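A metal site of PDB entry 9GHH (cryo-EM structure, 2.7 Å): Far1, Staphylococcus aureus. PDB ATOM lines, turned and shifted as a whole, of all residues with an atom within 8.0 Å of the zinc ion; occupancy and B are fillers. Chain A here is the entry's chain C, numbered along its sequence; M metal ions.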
ATOM      1  N   PHE A 119      26.065   3.139 -19.282  1.00  0.00           N
ATOM      2  CA  PHE A 119      25.490   2.510 -18.108  1.00  0.00           C
ATOM      3  C   PHE A 119      26.340   1.287 -17.737  1.00  0.00           C
ATOM      4  O   PHE A 119      27.059   0.760 -18.574  1.00  0.00           O
ATOM      5  CB  PHE A 119      24.039   2.113 -18.389  1.00  0.00           C
ATOM      6  CG  PHE A 119      23.883   1.063 -19.489  1.00  0.00           C
ATOM      7  CD1 PHE A 119      23.733   1.436 -20.824  1.00  0.00           C
ATOM      8  CD2 PHE A 119      23.873  -0.296 -19.188  1.00  0.00           C
ATOM      9  CE1 PHE A 119      23.594   0.476 -21.814  1.00  0.00           C
ATOM     10  CE2 PHE A 119      23.738  -1.243 -20.183  1.00  0.00           C
ATOM     11  CZ  PHE A 119      23.596  -0.855 -21.492  1.00  0.00           C
ATOM     12  N   GLY A 155      20.193 -11.390 -32.144  1.00  0.00           N
ATOM     13  CA  GLY A 155      18.935 -10.680 -32.305  1.00  0.00           C
ATOM     14  C   GLY A 155      19.114  -9.173 -32.131  1.00  0.00           C
ATOM     15  O   GLY A 155      20.074  -8.730 -31.510  1.00  0.00           O
ATOM     16  N   PHE A 156      18.178  -8.399 -32.685  1.00  0.00           N
ATOM     17  CA  PHE A 156      18.208  -6.948 -32.573  1.00  0.00           C
ATOM     18  C   PHE A 156      17.917  -6.581 -31.121  1.00  0.00           C
ATOM     19  O   PHE A 156      16.944  -7.065 -30.532  1.00  0.00           O
ATOM     20  CB  PHE A 156      17.219  -6.277 -33.531  1.00  0.00           C
ATOM     21  CG  PHE A 156      17.487  -4.790 -33.761  1.00  0.00           C
ATOM     22  CD1 PHE A 156      18.308  -4.368 -34.810  1.00  0.00           C
ATOM     23  CD2 PHE A 156      16.920  -3.820 -32.936  1.00  0.00           C
ATOM     24  CE1 PHE A 156      18.546  -3.027 -35.016  1.00  0.00           C
ATOM     25  CE2 PHE A 156      17.168  -2.470 -33.154  1.00  0.00           C
ATOM     26  CZ  PHE A 156      17.981  -2.074 -34.194  1.00  0.00           C
ATOM     27  N   CYS A 157      18.772  -5.724 -30.548  1.00  0.00           N
ATOM     28  CA  CYS A 157      18.710  -5.365 -29.143  1.00  0.00           C
ATOM     29  C   CYS A 157      18.239  -3.920 -29.010  1.00  0.00           C
ATOM     30  O   CYS A 157      18.789  -3.021 -29.647  1.00  0.00           O
ATOM     31  CB  CYS A 157      20.058  -5.569 -28.472  1.00  0.00           C
ATOM     32  SG  CYS A 157      20.175  -4.863 -26.812  1.00  0.00           S
ATOM     33  N   THR A 158      17.234  -3.708 -28.155  1.00  0.00           N
ATOM     34  CA  THR A 158      16.626  -2.400 -27.974  1.00  0.00           C
ATOM     35  C   THR A 158      17.599  -1.450 -27.285  1.00  0.00           C
ATOM     36  O   THR A 158      17.612  -0.256 -27.584  1.00  0.00           O
ATOM     37  CB  THR A 158      15.325  -2.534 -27.172  1.00  0.00           C
ATOM     38  OG1 THR A 158      14.496  -3.413 -27.933  1.00  0.00           O
ATOM     39  CG2 THR A 158      14.618  -1.209 -26.963  1.00  0.00           C
ATOM     40  N   ILE A 159      18.406  -1.986 -26.363  1.00  0.00           N
ATOM     41  CA  ILE A 159      19.253  -1.152 -25.520  1.00  0.00           C
ATOM     42  C   ILE A 159      20.261  -0.426 -26.420  1.00  0.00           C
ATOM     43  O   ILE A 159      20.381   0.798 -26.341  1.00  0.00           O
ATOM     44  CB  ILE A 159      19.949  -1.932 -24.397  1.00  0.00           C
ATOM     45  CG1 ILE A 159      19.067  -3.017 -23.770  1.00  0.00           C
ATOM     46  CG2 ILE A 159      20.479  -0.971 -23.339  1.00  0.00           C
ATOM     47  CD1 ILE A 159      19.667  -3.707 -22.564  1.00  0.00           C
ATOM     48  N   CYS A 160      20.957  -1.193 -27.269  1.00  0.00           N
ATOM     49  CA  CYS A 160      22.004  -0.640 -28.120  1.00  0.00           C
ATOM     50  C   CYS A 160      21.477  -0.275 -29.506  1.00  0.00           C
ATOM     51  O   CYS A 160      22.158   0.418 -30.254  1.00  0.00           O
ATOM     52  CB  CYS A 160      23.179  -1.596 -28.245  1.00  0.00           C
ATOM     53  SG  CYS A 160      22.719  -3.284 -28.711  1.00  0.00           S
ATOM     54  N   ASN A 161      20.263  -0.737 -29.834  1.00  0.00           N
ATOM     55  CA  ASN A 161      19.658  -0.507 -31.143  1.00  0.00           C
ATOM     56  C   ASN A 161      20.505  -1.160 -32.237  1.00  0.00           C
ATOM     57  O   ASN A 161      20.664  -0.598 -33.319  1.00  0.00           O
ATOM     58  CB  ASN A 161      19.444   0.985 -31.413  1.00  0.00           C
ATOM     59  CG  ASN A 161      18.695   1.673 -30.294  1.00  0.00           C
ATOM     60  OD1 ASN A 161      19.146   1.628 -29.139  1.00  0.00           O
ATOM     61  ND2 ASN A 161      17.568   2.299 -30.598  1.00  0.00           N
ATOM     62  N   LYS A 162      21.017  -2.365 -31.945  1.00  0.00           N
ATOM     63  CA  LYS A 162      21.859  -3.107 -32.882  1.00  0.00           C
ATOM     64  C   LYS A 162      21.475  -4.586 -32.851  1.00  0.00           C
ATOM     65  O   LYS A 162      20.902  -5.063 -31.876  1.00  0.00           O
ATOM     66  CB  LYS A 162      23.344  -3.002 -32.514  1.00  0.00           C
ATOM     67  CG  LYS A 162      23.914  -1.608 -32.370  1.00  0.00           C
ATOM     68  CD  LYS A 162      23.874  -0.749 -33.636  1.00  0.00           C
ATOM     69  CE  LYS A 162      24.418   0.636 -33.411  1.00  0.00           C
ATOM     70  NZ  LYS A 162      23.692   1.366 -32.369  1.00  0.00           N
ATOM     71  N   GLU A 163      21.817  -5.303 -33.935  1.00  0.00           N
ATOM     72  CA  GLU A 163      21.576  -6.737 -34.047  1.00  0.00           C
ATOM     73  C   GLU A 163      22.865  -7.480 -33.693  1.00  0.00           C
ATOM     74  O   GLU A 163      23.877  -7.318 -34.379  1.00  0.00           O
ATOM     75  CB  GLU A 163      21.066  -7.078 -35.443  1.00  0.00           C
ATOM     76  CG  GLU A 163      20.201  -8.346 -35.506  1.00  0.00           C
ATOM     77  CD  GLU A 163      20.913  -9.677 -35.391  1.00  0.00           C
ATOM     78  OE1 GLU A 163      22.159  -9.712 -35.405  1.00  0.00           O
ATOM     79  OE2 GLU A 163      20.200 -10.697 -35.297  1.00  0.00           O
ATOM     80  N   SER A 164      22.801  -8.292 -32.640  1.00  0.00           N
ATOM     81  CA  SER A 164      23.938  -9.078 -32.166  1.00  0.00           C
ATOM     82  C   SER A 164      23.443 -10.214 -31.280  1.00  0.00           C
ATOM     83  O   SER A 164      22.261 -10.283 -30.966  1.00  0.00           O
ATOM     84  CB  SER A 164      24.933  -8.214 -31.438  1.00  0.00           C
ATOM     85  OG  SER A 164      25.502  -7.239 -32.299  1.00  0.00           O
ATOM     86  N   ASN A 165      24.359 -11.097 -30.868  1.00  0.00           N
ATOM     87  CA  ASN A 165      24.030 -12.163 -29.930  1.00  0.00           C
ATOM     88  C   ASN A 165      23.521 -11.534 -28.627  1.00  0.00           C
ATOM     89  O   ASN A 165      24.186 -10.670 -28.060  1.00  0.00           O
ATOM     90  CB  ASN A 165      25.190 -13.126 -29.705  1.00  0.00           C
ATOM     91  CG  ASN A 165      26.398 -12.455 -29.091  1.00  0.00           C
ATOM     92  OD1 ASN A 165      26.988 -11.561 -29.710  1.00  0.00           O
ATOM     93  ND2 ASN A 165      26.778 -12.859 -27.887  1.00  0.00           N
ATOM     94  N   VAL A 166      22.345 -11.986 -28.179  1.00  0.00           N
ATOM     95  CA  VAL A 166      21.643 -11.350 -27.078  1.00  0.00           C
ATOM     96  C   VAL A 166      21.033 -12.444 -26.190  1.00  0.00           C
ATOM     97  O   VAL A 166      20.784 -13.558 -26.649  1.00  0.00           O
ATOM     98  CB  VAL A 166      20.575 -10.366 -27.591  1.00  0.00           C
ATOM     99  CG1 VAL A 166      21.191  -9.053 -28.054  1.00  0.00           C
ATOM    100  CG2 VAL A 166      19.718 -10.960 -28.707  1.00  0.00           C
ATOM    101  N   TYR A 187      15.234  -9.600 -25.655  1.00  0.00           N
ATOM    102  CA  TYR A 187      16.595 -10.080 -25.719  1.00  0.00           C
ATOM    103  C   TYR A 187      17.558  -8.898 -25.658  1.00  0.00           C
ATOM    104  O   TYR A 187      17.395  -7.934 -26.403  1.00  0.00           O
ATOM    105  CB  TYR A 187      16.793 -10.917 -26.990  1.00  0.00           C
ATOM    106  CG  TYR A 187      16.569 -12.417 -26.844  1.00  0.00           C
ATOM    107  CD1 TYR A 187      15.319 -12.992 -27.022  1.00  0.00           C
ATOM    108  CD2 TYR A 187      17.637 -13.257 -26.552  1.00  0.00           C
ATOM    109  CE1 TYR A 187      15.132 -14.359 -26.886  1.00  0.00           C
ATOM    110  CE2 TYR A 187      17.454 -14.630 -26.410  1.00  0.00           C
ATOM    111  CZ  TYR A 187      16.200 -15.182 -26.592  1.00  0.00           C
ATOM    112  OH  TYR A 187      16.019 -16.526 -26.452  1.00  0.00           O
ATOM    113  N   ILE A 188      18.551  -8.980 -24.757  1.00  0.00           N
ATOM    114  CA  ILE A 188      19.529  -7.922 -24.555  1.00  0.00           C
ATOM    115  C   ILE A 188      20.925  -8.539 -24.623  1.00  0.00           C
ATOM    116  O   ILE A 188      21.091  -9.728 -24.375  1.00  0.00           O
ATOM    117  CB  ILE A 188      19.274  -7.175 -23.234  1.00  0.00           C
ATOM    118  CG1 ILE A 188      19.786  -7.967 -22.018  1.00  0.00           C
ATOM    119  CG2 ILE A 188      17.803  -6.791 -23.097  1.00  0.00           C
ATOM    120  CD1 ILE A 188      19.744  -7.187 -20.710  1.00  0.00           C
ATOM    121  N   CYS A 189      21.930  -7.713 -24.938  1.00  0.00           N
ATOM    122  CA  CYS A 189      23.303  -8.188 -25.064  1.00  0.00           C
ATOM    123  C   CYS A 189      23.781  -8.721 -23.725  1.00  0.00           C
ATOM    124  O   CYS A 189      23.489  -8.135 -22.678  1.00  0.00           O
ATOM    125  CB  CYS A 189      24.230  -7.084 -25.560  1.00  0.00           C
ATOM    126  SG  CYS A 189      23.719  -6.334 -27.121  1.00  0.00           S
ATOM    127  N   ARG A 190      24.506  -9.849 -23.749  1.00  0.00           N
ATOM    128  CA  ARG A 190      24.928 -10.531 -22.541  1.00  0.00           C
ATOM    129  C   ARG A 190      25.886  -9.637 -21.762  1.00  0.00           C
ATOM    130  O   ARG A 190      25.817  -9.569 -20.534  1.00  0.00           O
ATOM    131  CB  ARG A 190      25.548 -11.896 -22.845  1.00  0.00           C
ATOM    132  CG  ARG A 190      25.668 -12.778 -21.617  1.00  0.00           C
ATOM    133  CD  ARG A 190      26.209 -14.171 -21.935  1.00  0.00           C
ATOM    134  NE  ARG A 190      26.057 -15.081 -20.793  1.00  0.00           N
ATOM    135  CZ  ARG A 190      24.904 -15.552 -20.316  1.00  0.00           C
ATOM    136  NH1 ARG A 190      23.758 -15.320 -20.937  1.00  0.00           N
ATOM    137  NH2 ARG A 190      24.902 -16.279 -19.214  1.00  0.00           N
ATOM    138  N   ASP A 191      26.789  -8.964 -22.488  1.00  0.00           N
ATOM    139  CA  ASP A 191      27.725  -8.021 -21.891  1.00  0.00           C
ATOM    140  C   ASP A 191      27.155  -6.615 -22.029  1.00  0.00           C
ATOM    141  O   ASP A 191      26.830  -6.181 -23.128  1.00  0.00           O
ATOM    142  CB  ASP A 191      29.116  -8.165 -22.504  1.00  0.00           C
ATOM    143  CG  ASP A 191      30.222  -7.371 -21.832  1.00  0.00           C
ATOM    144  OD1 ASP A 191      29.956  -6.734 -20.796  1.00  0.00           O
ATOM    145  OD2 ASP A 191      31.354  -7.385 -22.367  1.00  0.00           O
ATOM    146  N   SER A 192      27.045  -5.910 -20.891  1.00  0.00           N
ATOM    147  CA  SER A 192      26.555  -4.538 -20.866  1.00  0.00           C
ATOM    148  C   SER A 192      27.570  -3.609 -21.509  1.00  0.00           C
ATOM    149  O   SER A 192      27.192  -2.613 -22.129  1.00  0.00           O
ATOM    150  CB  SER A 192      26.237  -4.108 -19.458  1.00  0.00           C
ATOM    151  OG  SER A 192      25.231  -4.933 -18.883  1.00  0.00           O
ATOM    152  N   HIS A 194      29.691  -4.430 -23.947  1.00  0.00           N
ATOM    153  CA  HIS A 194      29.502  -4.657 -25.367  1.00  0.00           C
ATOM    154  C   HIS A 194      28.299  -3.854 -25.846  1.00  0.00           C
ATOM    155  O   HIS A 194      28.368  -3.195 -26.886  1.00  0.00           O
ATOM    156  CB  HIS A 194      29.334  -6.157 -25.661  1.00  0.00           C
ATOM    157  CG  HIS A 194      29.015  -6.465 -27.087  1.00  0.00           C
ATOM    158  ND1 HIS A 194      28.172  -7.492 -27.456  1.00  0.00           N
ATOM    159  CD2 HIS A 194      29.417  -5.890 -28.232  1.00  0.00           C
ATOM    160  CE1 HIS A 194      28.068  -7.533 -28.771  1.00  0.00           C
ATOM    161  NE2 HIS A 194      28.823  -6.573 -29.267  1.00  0.00           N
ATOM    162  N   CYS A 195      27.205  -3.923 -25.082  1.00  0.00           N
ATOM    163  CA  CYS A 195      25.991  -3.176 -25.384  1.00  0.00           C
ATOM    164  C   CYS A 195      26.279  -1.676 -25.414  1.00  0.00           C
ATOM    165  O   CYS A 195      25.779  -0.969 -26.282  1.00  0.00           O
ATOM    166  CB  CYS A 195      24.903  -3.488 -24.363  1.00  0.00           C
ATOM    167  SG  CYS A 195      23.267  -2.907 -24.862  1.00  0.00           S
ATOM    168  N   ASN A 196      27.092  -1.220 -24.456  1.00  0.00           N
ATOM    169  CA  ASN A 196      27.461   0.193 -24.361  1.00  0.00           C
ATOM    170  C   ASN A 196      28.267   0.623 -25.591  1.00  0.00           C
ATOM    171  O   ASN A 196      28.043   1.706 -26.107  1.00  0.00           O
ATOM    172  CB  ASN A 196      28.228   0.479 -23.075  1.00  0.00           C
ATOM    173  CG  ASN A 196      27.320   0.650 -21.891  1.00  0.00           C
ATOM    174  OD1 ASN A 196      26.568   1.623 -21.822  1.00  0.00           O
ATOM    175  ND2 ASN A 196      27.371  -0.273 -20.936  1.00  0.00           N
ATOM    176  N   LYS A 197      29.197  -0.233 -26.024  1.00  0.00           N
ATOM    177  CA  LYS A 197      30.028   0.066 -27.185  1.00  0.00           C
ATOM    178  C   LYS A 197      29.167   0.189 -28.439  1.00  0.00           C
ATOM    179  O   LYS A 197      29.408   1.044 -29.277  1.00  0.00           O
ATOM    180  CB  LYS A 197      31.107  -1.014 -27.362  1.00  0.00           C
ATOM    181  CG  LYS A 197      32.170  -1.030 -26.270  1.00  0.00           C
ATOM    182  CD  LYS A 197      33.158  -2.182 -26.375  1.00  0.00           C
ATOM    183  CE  LYS A 197      34.191  -2.140 -25.299  1.00  0.00           C
ATOM    184  NZ  LYS A 197      35.141  -3.251 -25.388  1.00  0.00           N
ATOM    185  N   GLN A 198      28.160  -0.688 -28.536  1.00  0.00           N
ATOM    186  CA  GLN A 198      27.202  -0.656 -29.628  1.00  0.00           C
ATOM    187  C   GLN A 198      26.333   0.596 -29.536  1.00  0.00           C
ATOM    188  O   GLN A 198      26.007   1.200 -30.558  1.00  0.00           O
ATOM    189  CB  GLN A 198      26.335  -1.922 -29.584  1.00  0.00           C
ATOM    190  CG  GLN A 198      27.083  -3.209 -29.868  1.00  0.00           C
ATOM    191  CD  GLN A 198      26.281  -4.440 -29.508  1.00  0.00           C
ATOM    192  OE1 GLN A 198      25.923  -4.656 -28.351  1.00  0.00           O
ATOM    193  NE2 GLN A 198      25.994  -5.265 -30.508  1.00  0.00           N
ATOM    194  N   LEU A 199      25.955   0.960 -28.311  1.00  0.00           N
ATOM    195  CA  LEU A 199      25.108   2.119 -28.051  1.00  0.00           C
ATOM    196  C   LEU A 199      25.816   3.397 -28.508  1.00  0.00           C
ATOM    197  O   LEU A 199      26.996   3.574 -28.215  1.00  0.00           O
ATOM    198  CB  LEU A 199      24.766   2.154 -26.564  1.00  0.00           C
ATOM    199  CG  LEU A 199      23.812   3.257 -26.116  1.00  0.00           C
ATOM    200  CD1 LEU A 199      22.453   3.054 -26.774  1.00  0.00           C
ATOM    201  CD2 LEU A 199      23.673   3.295 -24.606  1.00  0.00           C
ATOM    202  N   PHE A 208      14.860   2.271 -23.953  1.00  0.00           N
ATOM    203  CA  PHE A 208      14.744   0.882 -23.546  1.00  0.00           C
ATOM    204  C   PHE A 208      14.173   0.813 -22.124  1.00  0.00           C
ATOM    205  O   PHE A 208      13.310  -0.011 -21.857  1.00  0.00           O
ATOM    206  CB  PHE A 208      16.085   0.146 -23.638  1.00  0.00           C
ATOM    207  CG  PHE A 208      16.154  -1.140 -22.827  1.00  0.00           C
ATOM    208  CD1 PHE A 208      15.617  -2.328 -23.315  1.00  0.00           C
ATOM    209  CD2 PHE A 208      16.769  -1.155 -21.583  1.00  0.00           C
ATOM    210  CE1 PHE A 208      15.694  -3.493 -22.569  1.00  0.00           C
ATOM    211  CE2 PHE A 208      16.844  -2.330 -20.847  1.00  0.00           C
ATOM    212  CZ  PHE A 208      16.306  -3.500 -21.333  1.00  0.00           C
HETATM  213 ZN    ZN M   1      22.477  -4.362 -26.532  1.00  0.00          ZN
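Merely in contact with the zinc ion: Gln 198. Within 4 Å of the zinc ion: Cys 157, Cys 160, Cys 189, Cys 195 and Gln 198.
The zinc ion is bound by SG of Cys 195, SG of Cys 157, SG of Cys 189 and SG of Cys 160.
SG of Cys 157 sits close to N of Ile 159. The backbone NH (N) of Cys 157 sits at hydrogen-bond distance from the backbone carbonyl oxygen (O) of Lys 162. SG of Cys 189 lies close to OE1 of Gln 198 (3.0 Å). OE1 of Gln 198 sits close to SG of Cys 160 (3.5 Å). O of Cys 160 is in hydrogen-bond range of NZ of Lys 162 (2.8 Å). NZ of Lys 162 is in hydrogen-bond range of O of Gln 198, 2.9 Å away. OE1 of Gln 198 sits close to O of His 194, at 3.2 Å. The side-chain amide nitrogen of Gln 198 lies within hydrogen-bond range of the side-chain hydroxyl of Ser 164 (2.7 Å).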
